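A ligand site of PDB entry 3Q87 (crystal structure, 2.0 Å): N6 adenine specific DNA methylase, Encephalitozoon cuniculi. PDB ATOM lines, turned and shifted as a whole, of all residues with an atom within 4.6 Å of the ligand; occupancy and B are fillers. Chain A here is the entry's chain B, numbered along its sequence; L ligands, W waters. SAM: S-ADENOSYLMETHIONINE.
A nitrogen (N3) of the ligand lies within hydrogen-bond range of the backbone NH (N) of Leu 52 (3.4 Å).
O of Gly 31 lies within hydrogen-bond range of N of the ligand, 2.7 Å away.
The side-chain carboxylate of Asp 69 sits at hydrogen-bond distance from a nitrogen (N6) of the ligand (2.9 Å).
ND2 of Asn 85 sits at hydrogen-bond distance from OXT of the ligand (3.0 Å).
OD2 of Asp 51 is in hydrogen-bond range of O2' of the ligand, at 2.6 Å.
The backbone NH (N) of Leu 70 lies within hydrogen-bond range of a nitrogen (N1) of the ligand (2.9 Å).
N of Ser 33 is in hydrogen-bond range of OD1 of Asp 51 (2.7 Å).
N of Ala 68 lies within hydrogen-bond range of O of Asp 51 (3.1 Å).
The side-chain carboxylate (OD1) of Asp 51 is in hydrogen-bond range of the backbone NH (N) of Thr 32, at 3.3 Å.
The backbone carbonyl oxygen (O) of Tyr 4 sits at hydrogen-bond distance from the side-chain hydroxyl (OG) of Ser 33.
OD1 of Asp 69 lies within salt-bridge range of NH2 of Arg 109.
The side-chain hydroxyl (OG1) of Thr 32 lies within hydrogen-bond range of the side-chain carboxylate (OD2) of Asp 29 (2.9 Å).
The side-chain carboxylate (OD2) of Asp 51 sits at hydrogen-bond distance from the backbone NH (N) of Asn 53.
Tyr 4 touches the ligand.
CG2 of Thr 10 touches O of the ligand, at 2.8 Å.
Thr 32 touches the ligand.
Ser 33 touches the ligand.
Ile 37 touches the ligand.
CB of Asn 53 touches O2' of the ligand (3.5 Å).
Ala 68 touches the ligand.
Pro 86 touches the ligand.
CG of Pro 87 touches C8 of the ligand, 3.3 Å away.
Pro 95 touches the ligand (O to C8, 3.3 Å).
Ile 96 touches the ligand.
Water W7 bridges an oxygen (O) of the ligand (2.4 Å) and the backbone carbonyl oxygen (O) of Tyr 4 (3.2 Å).
Water W1 lies within hydrogen-bond range of O3' of the ligand (2.8 Å), N of Tyr 4 (3.0 Å), ND2 of Asn 53 (3.1 Å) and OG of Ser 33 (3.1 Å).
Water W4 lies within hydrogen-bond range of N7 of the ligand and O of Pro 95.
Water W8 bridges O of Pro 95 and O2' of the ligand.
Water W3 bridges a nitrogen (N6) of the ligand (2.9 Å) and the guanidinium group of Arg 109 (3.0 Å).
Water W5 lies within hydrogen-bond range of the backbone carbonyl oxygen of Thr 32 (2.8 Å), the side-chain carboxylate of Asp 29 (2.9 Å), the backbone NH of Ile 37 (3.0 Å), a nitrogen (N) of the ligand (3.4 Å) and the backbone NH of Val 36 (3.5 Å).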
ATOM      1  N   TYR A   4      14.862 -13.750   6.591  1.00  0.00           N
ATOM      2  CA  TYR A   4      15.269 -14.553   7.732  1.00  0.00           C
ATOM      3  C   TYR A   4      16.034 -15.784   7.266  1.00  0.00           C
ATOM      4  O   TYR A   4      15.546 -16.549   6.440  1.00  0.00           O
ATOM      5  CB  TYR A   4      14.033 -14.973   8.528  1.00  0.00           C
ATOM      6  CG  TYR A   4      14.367 -15.501   9.911  1.00  0.00           C
ATOM      7  CD1 TYR A   4      14.510 -14.621  10.987  1.00  0.00           C
ATOM      8  CD2 TYR A   4      14.543 -16.853  10.137  1.00  0.00           C
ATOM      9  CE1 TYR A   4      14.818 -15.071  12.240  1.00  0.00           C
ATOM     10  CE2 TYR A   4      14.863 -17.323  11.416  1.00  0.00           C
ATOM     11  CZ  TYR A   4      14.994 -16.423  12.466  1.00  0.00           C
ATOM     12  OH  TYR A   4      15.298 -16.860  13.738  1.00  0.00           O
ATOM     13  N   GLU A   5      17.223 -15.994   7.816  1.00  0.00           N
ATOM     14  CA  GLU A   5      18.077 -17.092   7.389  1.00  0.00           C
ATOM     15  C   GLU A   5      17.949 -18.262   8.366  1.00  0.00           C
ATOM     16  O   GLU A   5      17.647 -18.048   9.531  1.00  0.00           O
ATOM     17  CB  GLU A   5      19.526 -16.609   7.300  1.00  0.00           C
ATOM     18  CG  GLU A   5      19.729 -15.523   6.278  1.00  0.00           C
ATOM     19  CD  GLU A   5      21.061 -14.796   6.442  1.00  0.00           C
ATOM     20  OE1 GLU A   5      21.935 -15.298   7.189  1.00  0.00           O
ATOM     21  OE2 GLU A   5      21.220 -13.711   5.836  1.00  0.00           O
ATOM     22  N   PRO A   6      18.192 -19.503   7.890  1.00  0.00           N
ATOM     23  CA  PRO A   6      18.062 -20.671   8.769  1.00  0.00           C
ATOM     24  C   PRO A   6      18.941 -20.558  10.011  1.00  0.00           C
ATOM     25  O   PRO A   6      20.125 -20.257   9.871  1.00  0.00           O
ATOM     26  CB  PRO A   6      18.547 -21.827   7.881  1.00  0.00           C
ATOM     27  CG  PRO A   6      18.297 -21.336   6.478  1.00  0.00           C
ATOM     28  CD  PRO A   6      18.563 -19.872   6.509  1.00  0.00           C
ATOM     29  N   THR A  10      15.102 -22.677  13.497  1.00  0.00           N
ATOM     30  CA  THR A  10      14.533 -23.419  12.368  1.00  0.00           C
ATOM     31  C   THR A  10      14.918 -24.899  12.451  1.00  0.00           C
ATOM     32  O   THR A  10      14.092 -25.763  12.243  1.00  0.00           O
ATOM     33  CB  THR A  10      14.911 -22.827  10.979  1.00  0.00           C
ATOM     34  OG1 THR A  10      15.764 -23.725  10.264  1.00  0.00           O
ATOM     35  CG2 THR A  10      15.585 -21.477  11.093  1.00  0.00           C
ATOM     36  N   ASP A  29       3.695 -24.407   4.369  1.00  0.00           N
ATOM     37  CA  ASP A  29       4.872 -23.878   5.059  1.00  0.00           C
ATOM     38  C   ASP A  29       4.687 -22.358   5.148  1.00  0.00           C
ATOM     39  O   ASP A  29       4.999 -21.621   4.207  1.00  0.00           O
ATOM     40  CB  ASP A  29       6.157 -24.204   4.280  1.00  0.00           C
ATOM     41  CG  ASP A  29       7.412 -23.589   4.907  1.00  0.00           C
ATOM     42  OD1 ASP A  29       7.349 -23.081   6.059  1.00  0.00           O
ATOM     43  OD2 ASP A  29       8.480 -23.614   4.246  1.00  0.00           O
ATOM     44  N   LEU A  30       4.157 -21.905   6.270  1.00  0.00           N
ATOM     45  CA  LEU A  30       3.814 -20.507   6.477  1.00  0.00           C
ATOM     46  C   LEU A  30       5.050 -19.747   6.961  1.00  0.00           C
ATOM     47  O   LEU A  30       5.698 -20.188   7.901  1.00  0.00           O
ATOM     48  CB  LEU A  30       2.696 -20.436   7.518  1.00  0.00           C
ATOM     49  CG  LEU A  30       2.029 -19.100   7.834  1.00  0.00           C
ATOM     50  CD1 LEU A  30       1.404 -18.533   6.593  1.00  0.00           C
ATOM     51  CD2 LEU A  30       0.973 -19.302   8.921  1.00  0.00           C
ATOM     52  N   GLY A  31       5.355 -18.603   6.350  1.00  0.00           N
ATOM     53  CA  GLY A  31       6.597 -17.896   6.665  1.00  0.00           C
ATOM     54  C   GLY A  31       7.789 -18.731   6.186  1.00  0.00           C
ATOM     55  O   GLY A  31       8.737 -18.992   6.917  1.00  0.00           O
ATOM     56  N   THR A  32       7.722 -19.136   4.925  1.00  0.00           N
ATOM     57  CA  THR A  32       8.699 -20.056   4.370  1.00  0.00           C
ATOM     58  C   THR A  32      10.065 -19.426   4.263  1.00  0.00           C
ATOM     59  O   THR A  32      11.071 -20.134   4.227  1.00  0.00           O
ATOM     60  CB  THR A  32       8.265 -20.538   2.961  1.00  0.00           C
ATOM     61  OG1 THR A  32       9.239 -21.447   2.447  1.00  0.00           O
ATOM     62  CG2 THR A  32       8.122 -19.362   2.012  1.00  0.00           C
ATOM     63  N   SER A  33      10.109 -18.094   4.193  1.00  0.00           N
ATOM     64  CA  SER A  33      11.357 -17.377   3.913  1.00  0.00           C
ATOM     65  C   SER A  33      12.005 -17.912   2.624  1.00  0.00           C
ATOM     66  O   SER A  33      11.376 -17.873   1.557  1.00  0.00           O
ATOM     67  CB  SER A  33      12.309 -17.442   5.099  1.00  0.00           C
ATOM     68  OG  SER A  33      13.391 -16.545   4.911  1.00  0.00           O
ATOM     69  N   VAL A  36      13.994 -23.421   3.479  1.00  0.00           N
ATOM     70  CA  VAL A  36      14.733 -24.522   4.078  1.00  0.00           C
ATOM     71  C   VAL A  36      13.785 -25.618   4.595  1.00  0.00           C
ATOM     72  O   VAL A  36      14.041 -26.804   4.414  1.00  0.00           O
ATOM     73  CB  VAL A  36      15.724 -24.030   5.191  1.00  0.00           C
ATOM     74  CG1 VAL A  36      14.963 -23.629   6.481  1.00  0.00           C
ATOM     75  CG2 VAL A  36      16.781 -25.063   5.463  1.00  0.00           C
ATOM     76  N   ILE A  37      12.676 -25.231   5.207  1.00  0.00           N
ATOM     77  CA  ILE A  37      11.726 -26.238   5.693  1.00  0.00           C
ATOM     78  C   ILE A  37      10.915 -26.873   4.548  1.00  0.00           C
ATOM     79  O   ILE A  37      10.674 -28.097   4.536  1.00  0.00           O
ATOM     80  CB  ILE A  37      10.808 -25.663   6.778  1.00  0.00           C
ATOM     81  CG1 ILE A  37      11.651 -25.201   7.975  1.00  0.00           C
ATOM     82  CG2 ILE A  37       9.798 -26.703   7.226  1.00  0.00           C
ATOM     83  CD1 ILE A  37      10.805 -24.574   9.099  1.00  0.00           C
ATOM     84  N   ASP A  51       4.951 -16.384   2.235  1.00  0.00           N
ATOM     85  CA  ASP A  51       5.655 -15.418   3.064  1.00  0.00           C
ATOM     86  C   ASP A  51       5.165 -14.008   2.717  1.00  0.00           C
ATOM     87  O   ASP A  51       4.671 -13.761   1.617  1.00  0.00           O
ATOM     88  CB  ASP A  51       7.181 -15.503   2.846  1.00  0.00           C
ATOM     89  CG  ASP A  51       7.968 -15.055   4.073  1.00  0.00           C
ATOM     90  OD1 ASP A  51       8.604 -15.914   4.714  1.00  0.00           O
ATOM     91  OD2 ASP A  51       7.915 -13.862   4.416  1.00  0.00           O
ATOM     92  N   LEU A  52       5.265 -13.114   3.690  1.00  0.00           N
ATOM     93  CA  LEU A  52       4.954 -11.712   3.472  1.00  0.00           C
ATOM     94  C   LEU A  52       6.120 -11.036   2.737  1.00  0.00           C
ATOM     95  O   LEU A  52       5.942 -10.041   2.045  1.00  0.00           O
ATOM     96  CB  LEU A  52       4.706 -11.025   4.818  1.00  0.00           C
ATOM     97  CG  LEU A  52       4.164  -9.606   4.799  1.00  0.00           C
ATOM     98  CD1 LEU A  52       2.795  -9.606   4.097  1.00  0.00           C
ATOM     99  CD2 LEU A  52       4.039  -9.085   6.224  1.00  0.00           C
ATOM    100  N   ASN A  53       7.319 -11.609   2.897  1.00  0.00           N
ATOM    101  CA  ASN A  53       8.565 -11.026   2.402  1.00  0.00           C
ATOM    102  C   ASN A  53       8.908 -11.433   0.966  1.00  0.00           C
ATOM    103  O   ASN A  53       9.356 -12.559   0.712  1.00  0.00           O
ATOM    104  CB  ASN A  53       9.692 -11.430   3.375  1.00  0.00           C
ATOM    105  CG  ASN A  53      11.035 -10.890   2.967  1.00  0.00           C
ATOM    106  OD1 ASN A  53      11.182 -10.217   1.951  1.00  0.00           O
ATOM    107  ND2 ASN A  53      12.052 -11.195   3.772  1.00  0.00           N
ATOM    108  N   ALA A  68       1.687 -13.808   0.820  1.00  0.00           N
ATOM    109  CA  ALA A  68       0.413 -13.661   1.517  1.00  0.00           C
ATOM    110  C   ALA A  68       0.616 -13.260   2.961  1.00  0.00           C
ATOM    111  O   ALA A  68       1.671 -13.513   3.540  1.00  0.00           O
ATOM    112  CB  ALA A  68      -0.371 -14.964   1.460  1.00  0.00           C
ATOM    113  N   ASP A  69      -0.425 -12.659   3.546  1.00  0.00           N
ATOM    114  CA  ASP A  69      -0.427 -12.277   4.954  1.00  0.00           C
ATOM    115  C   ASP A  69      -1.138 -13.393   5.720  1.00  0.00           C
ATOM    116  O   ASP A  69      -2.360 -13.553   5.613  1.00  0.00           O
ATOM    117  CB  ASP A  69      -1.150 -10.926   5.106  1.00  0.00           C
ATOM    118  CG  ASP A  69      -0.973 -10.306   6.492  1.00  0.00           C
ATOM    119  OD1 ASP A  69      -0.625 -11.022   7.456  1.00  0.00           O
ATOM    120  OD2 ASP A  69      -1.196  -9.084   6.608  1.00  0.00           O
ATOM    121  N   LEU A  70      -0.370 -14.184   6.455  1.00  0.00           N
ATOM    122  CA  LEU A  70      -0.920 -15.359   7.131  1.00  0.00           C
ATOM    123  C   LEU A  70      -1.790 -16.186   6.168  1.00  0.00           C
ATOM    124  O   LEU A  70      -1.309 -16.573   5.113  1.00  0.00           O
ATOM    125  CB  LEU A  70      -1.683 -14.960   8.389  1.00  0.00           C
ATOM    126  CG  LEU A  70      -0.889 -14.275   9.510  1.00  0.00           C
ATOM    127  CD1 LEU A  70      -1.793 -14.054  10.726  1.00  0.00           C
ATOM    128  CD2 LEU A  70       0.332 -15.086   9.911  1.00  0.00           C
ATOM    129  N   PHE A  84       4.717 -23.395  10.985  1.00  0.00           N
ATOM    130  CA  PHE A  84       4.947 -21.958  11.122  1.00  0.00           C
ATOM    131  C   PHE A  84       6.045 -21.642  12.126  1.00  0.00           C
ATOM    132  O   PHE A  84       5.856 -21.805  13.326  1.00  0.00           O
ATOM    133  CB  PHE A  84       3.655 -21.274  11.560  1.00  0.00           C
ATOM    134  CG  PHE A  84       3.678 -19.771  11.447  1.00  0.00           C
ATOM    135  CD1 PHE A  84       4.603 -19.130  10.647  1.00  0.00           C
ATOM    136  CD2 PHE A  84       2.726 -19.002  12.113  1.00  0.00           C
ATOM    137  CE1 PHE A  84       4.602 -17.755  10.530  1.00  0.00           C
ATOM    138  CE2 PHE A  84       2.716 -17.622  11.997  1.00  0.00           C
ATOM    139  CZ  PHE A  84       3.647 -16.992  11.210  1.00  0.00           C
ATOM    140  N   ASN A  85       7.200 -21.199  11.650  1.00  0.00           N
ATOM    141  CA  ASN A  85       8.159 -20.521  12.510  1.00  0.00           C
ATOM    142  C   ASN A  85       7.849 -19.033  12.382  1.00  0.00           C
ATOM    143  O   ASN A  85       8.184 -18.421  11.380  1.00  0.00           O
ATOM    144  CB  ASN A  85       9.591 -20.849  12.107  1.00  0.00           C
ATOM    145  CG  ASN A  85      10.622 -20.228  13.045  1.00  0.00           C
ATOM    146  OD1 ASN A  85      10.279 -19.629  14.054  1.00  0.00           O
ATOM    147  ND2 ASN A  85      11.890 -20.371  12.698  1.00  0.00           N
ATOM    148  N   PRO A  86       7.167 -18.458  13.382  1.00  0.00           N
ATOM    149  CA  PRO A  86       6.603 -17.118  13.232  1.00  0.00           C
ATOM    150  C   PRO A  86       7.575 -16.008  13.644  1.00  0.00           C
ATOM    151  O   PRO A  86       8.590 -16.307  14.283  1.00  0.00           O
ATOM    152  CB  PRO A  86       5.419 -17.143  14.204  1.00  0.00           C
ATOM    153  CG  PRO A  86       5.905 -18.024  15.319  1.00  0.00           C
ATOM    154  CD  PRO A  86       6.864 -19.041  14.704  1.00  0.00           C
ATOM    155  N   PRO A  87       7.273 -14.747  13.265  1.00  0.00           N
ATOM    156  CA  PRO A  87       8.036 -13.599  13.818  1.00  0.00           C
ATOM    157  C   PRO A  87       7.716 -13.543  15.305  1.00  0.00           C
ATOM    158  O   PRO A  87       6.580 -13.273  15.659  1.00  0.00           O
ATOM    159  CB  PRO A  87       7.386 -12.377  13.164  1.00  0.00           C
ATOM    160  CG  PRO A  87       6.342 -12.887  12.224  1.00  0.00           C
ATOM    161  CD  PRO A  87       6.131 -14.337  12.436  1.00  0.00           C
ATOM    162  N   PRO A  95       9.089  -6.191  10.150  1.00  0.00           N
ATOM    163  CA  PRO A  95       8.145  -6.997   9.362  1.00  0.00           C
ATOM    164  C   PRO A  95       8.588  -8.449   9.246  1.00  0.00           C
ATOM    165  O   PRO A  95       7.760  -9.313   8.961  1.00  0.00           O
ATOM    166  CB  PRO A  95       8.164  -6.315   7.984  1.00  0.00           C
ATOM    167  CG  PRO A  95       8.633  -4.941   8.265  1.00  0.00           C
ATOM    168  CD  PRO A  95       9.649  -5.085   9.352  1.00  0.00           C
ATOM    169  N   ILE A  96       9.876  -8.726   9.464  1.00  0.00           N
ATOM    170  CA  ILE A  96      10.386 -10.094   9.344  1.00  0.00           C
ATOM    171  C   ILE A  96      10.386 -10.854  10.668  1.00  0.00           C
ATOM    172  O   ILE A  96       9.950 -11.997  10.724  1.00  0.00           O
ATOM    173  CB  ILE A  96      11.799 -10.105   8.705  1.00  0.00           C
ATOM    174  CG1 ILE A  96      11.766  -9.501   7.313  1.00  0.00           C
ATOM    175  CG2 ILE A  96      12.358 -11.529   8.612  1.00  0.00           C
ATOM    176  CD1 ILE A  96      13.160  -9.185   6.784  1.00  0.00           C
ATOM    177  N   VAL A 106       1.782 -11.580  16.003  1.00  0.00           N
ATOM    178  CA  VAL A 106       1.519 -12.380  14.812  1.00  0.00           C
ATOM    179  C   VAL A 106       1.044 -13.769  15.215  1.00  0.00           C
ATOM    180  O   VAL A 106       0.103 -14.311  14.641  1.00  0.00           O
ATOM    181  CB  VAL A 106       2.744 -12.458  13.864  1.00  0.00           C
ATOM    182  CG1 VAL A 106       2.374 -13.197  12.560  1.00  0.00           C
ATOM    183  CG2 VAL A 106       3.246 -11.068  13.519  1.00  0.00           C
ATOM    184  N   ARG A 109      -2.539 -13.560  16.075  1.00  0.00           N
ATOM    185  CA  ARG A 109      -3.336 -13.439  14.861  1.00  0.00           C
ATOM    186  C   ARG A 109      -3.482 -14.785  14.155  1.00  0.00           C
ATOM    187  O   ARG A 109      -4.555 -15.131  13.647  1.00  0.00           O
ATOM    188  CB  ARG A 109      -2.748 -12.391  13.912  1.00  0.00           C
ATOM    189  CG  ARG A 109      -3.128 -10.985  14.290  1.00  0.00           C
ATOM    190  CD  ARG A 109      -2.482  -9.926  13.409  1.00  0.00           C
ATOM    191  NE  ARG A 109      -2.687 -10.165  11.974  1.00  0.00           N
ATOM    192  CZ  ARG A 109      -1.691 -10.160  11.081  1.00  0.00           C
ATOM    193  NH1 ARG A 109      -0.449  -9.913  11.480  1.00  0.00           N
ATOM    194  NH2 ARG A 109      -1.933 -10.374   9.800  1.00  0.00           N
HETATM  195  N   SAM L   1      10.624 -20.648   7.924  1.00  0.00           N
HETATM  196  CA  SAM L   1      11.852 -19.863   8.096  1.00  0.00           C
HETATM  197  C   SAM L   1      12.787 -20.597   9.072  1.00  0.00           C
HETATM  198  O   SAM L   1      13.996 -20.396   9.091  1.00  0.00           O
HETATM  199  OXT SAM L   1      12.338 -21.406   9.878  1.00  0.00           O
HETATM  200  CB  SAM L   1      11.623 -18.375   8.493  1.00  0.00           C
HETATM  201  CG  SAM L   1      11.071 -17.974   9.889  1.00  0.00           C
HETATM  202  SD  SAM L   1      11.070 -16.178  10.336  1.00  0.00           S
HETATM  203  CE  SAM L   1      11.309 -16.218  12.121  1.00  0.00           C
HETATM  204  C5' SAM L   1       9.327 -15.728  10.245  1.00  0.00           C
HETATM  205  C4' SAM L   1       8.917 -15.605   8.783  1.00  0.00           C
HETATM  206  O4' SAM L   1       7.565 -15.198   8.689  1.00  0.00           O
HETATM  207  C3' SAM L   1       9.749 -14.578   8.016  1.00  0.00           C
HETATM  208  O3' SAM L   1      10.170 -15.174   6.810  1.00  0.00           O
HETATM  209  C2' SAM L   1       8.777 -13.451   7.733  1.00  0.00           C
HETATM  210  O2' SAM L   1       9.014 -12.792   6.501  1.00  0.00           O
HETATM  211  C1' SAM L   1       7.461 -14.180   7.708  1.00  0.00           C
HETATM  212  N9  SAM L   1       6.327 -13.360   8.078  1.00  0.00           N
HETATM  213  C8  SAM L   1       6.266 -12.284   8.933  1.00  0.00           C
HETATM  214  N7  SAM L   1       4.993 -11.856   8.974  1.00  0.00           N
HETATM  215  C5  SAM L   1       4.244 -12.655   8.164  1.00  0.00           C
HETATM  216  C6  SAM L   1       2.898 -12.698   7.832  1.00  0.00           C
HETATM  217  N6  SAM L   1       2.068 -11.808   8.358  1.00  0.00           N
HETATM  218  N1  SAM L   1       2.430 -13.667   6.962  1.00  0.00           N
HETATM  219  C2  SAM L   1       3.283 -14.612   6.405  1.00  0.00           C
HETATM  220  N3  SAM L   1       4.619 -14.568   6.751  1.00  0.00           N
HETATM  221  C4  SAM L   1       5.079 -13.609   7.594  1.00  0.00           C
HETATM  222  O   HOH W   1      12.125 -13.746   5.447  1.00  0.00           O
HETATM  223  O   HOH W   2       1.365 -16.450   4.480  1.00  0.00           O
HETATM  224  O   HOH W   3       1.992  -9.295   9.799  1.00  0.00           O
HETATM  225  O   HOH W   4       4.828  -9.357  10.203  1.00  0.00           O
HETATM  226  O   HOH W   5      11.046 -22.717   5.198  1.00  0.00           O
HETATM  227  O   HOH W   6      11.428 -14.454  14.796  1.00  0.00           O
HETATM  228  O   HOH W   7      15.006 -19.653   6.998  1.00  0.00           O
HETATM  229  O   HOH W   8       7.707 -10.275   6.469  1.00  0.00           O
HETATM  230  O   HOH W   9       7.742 -21.553   8.961  1.00  0.00           O
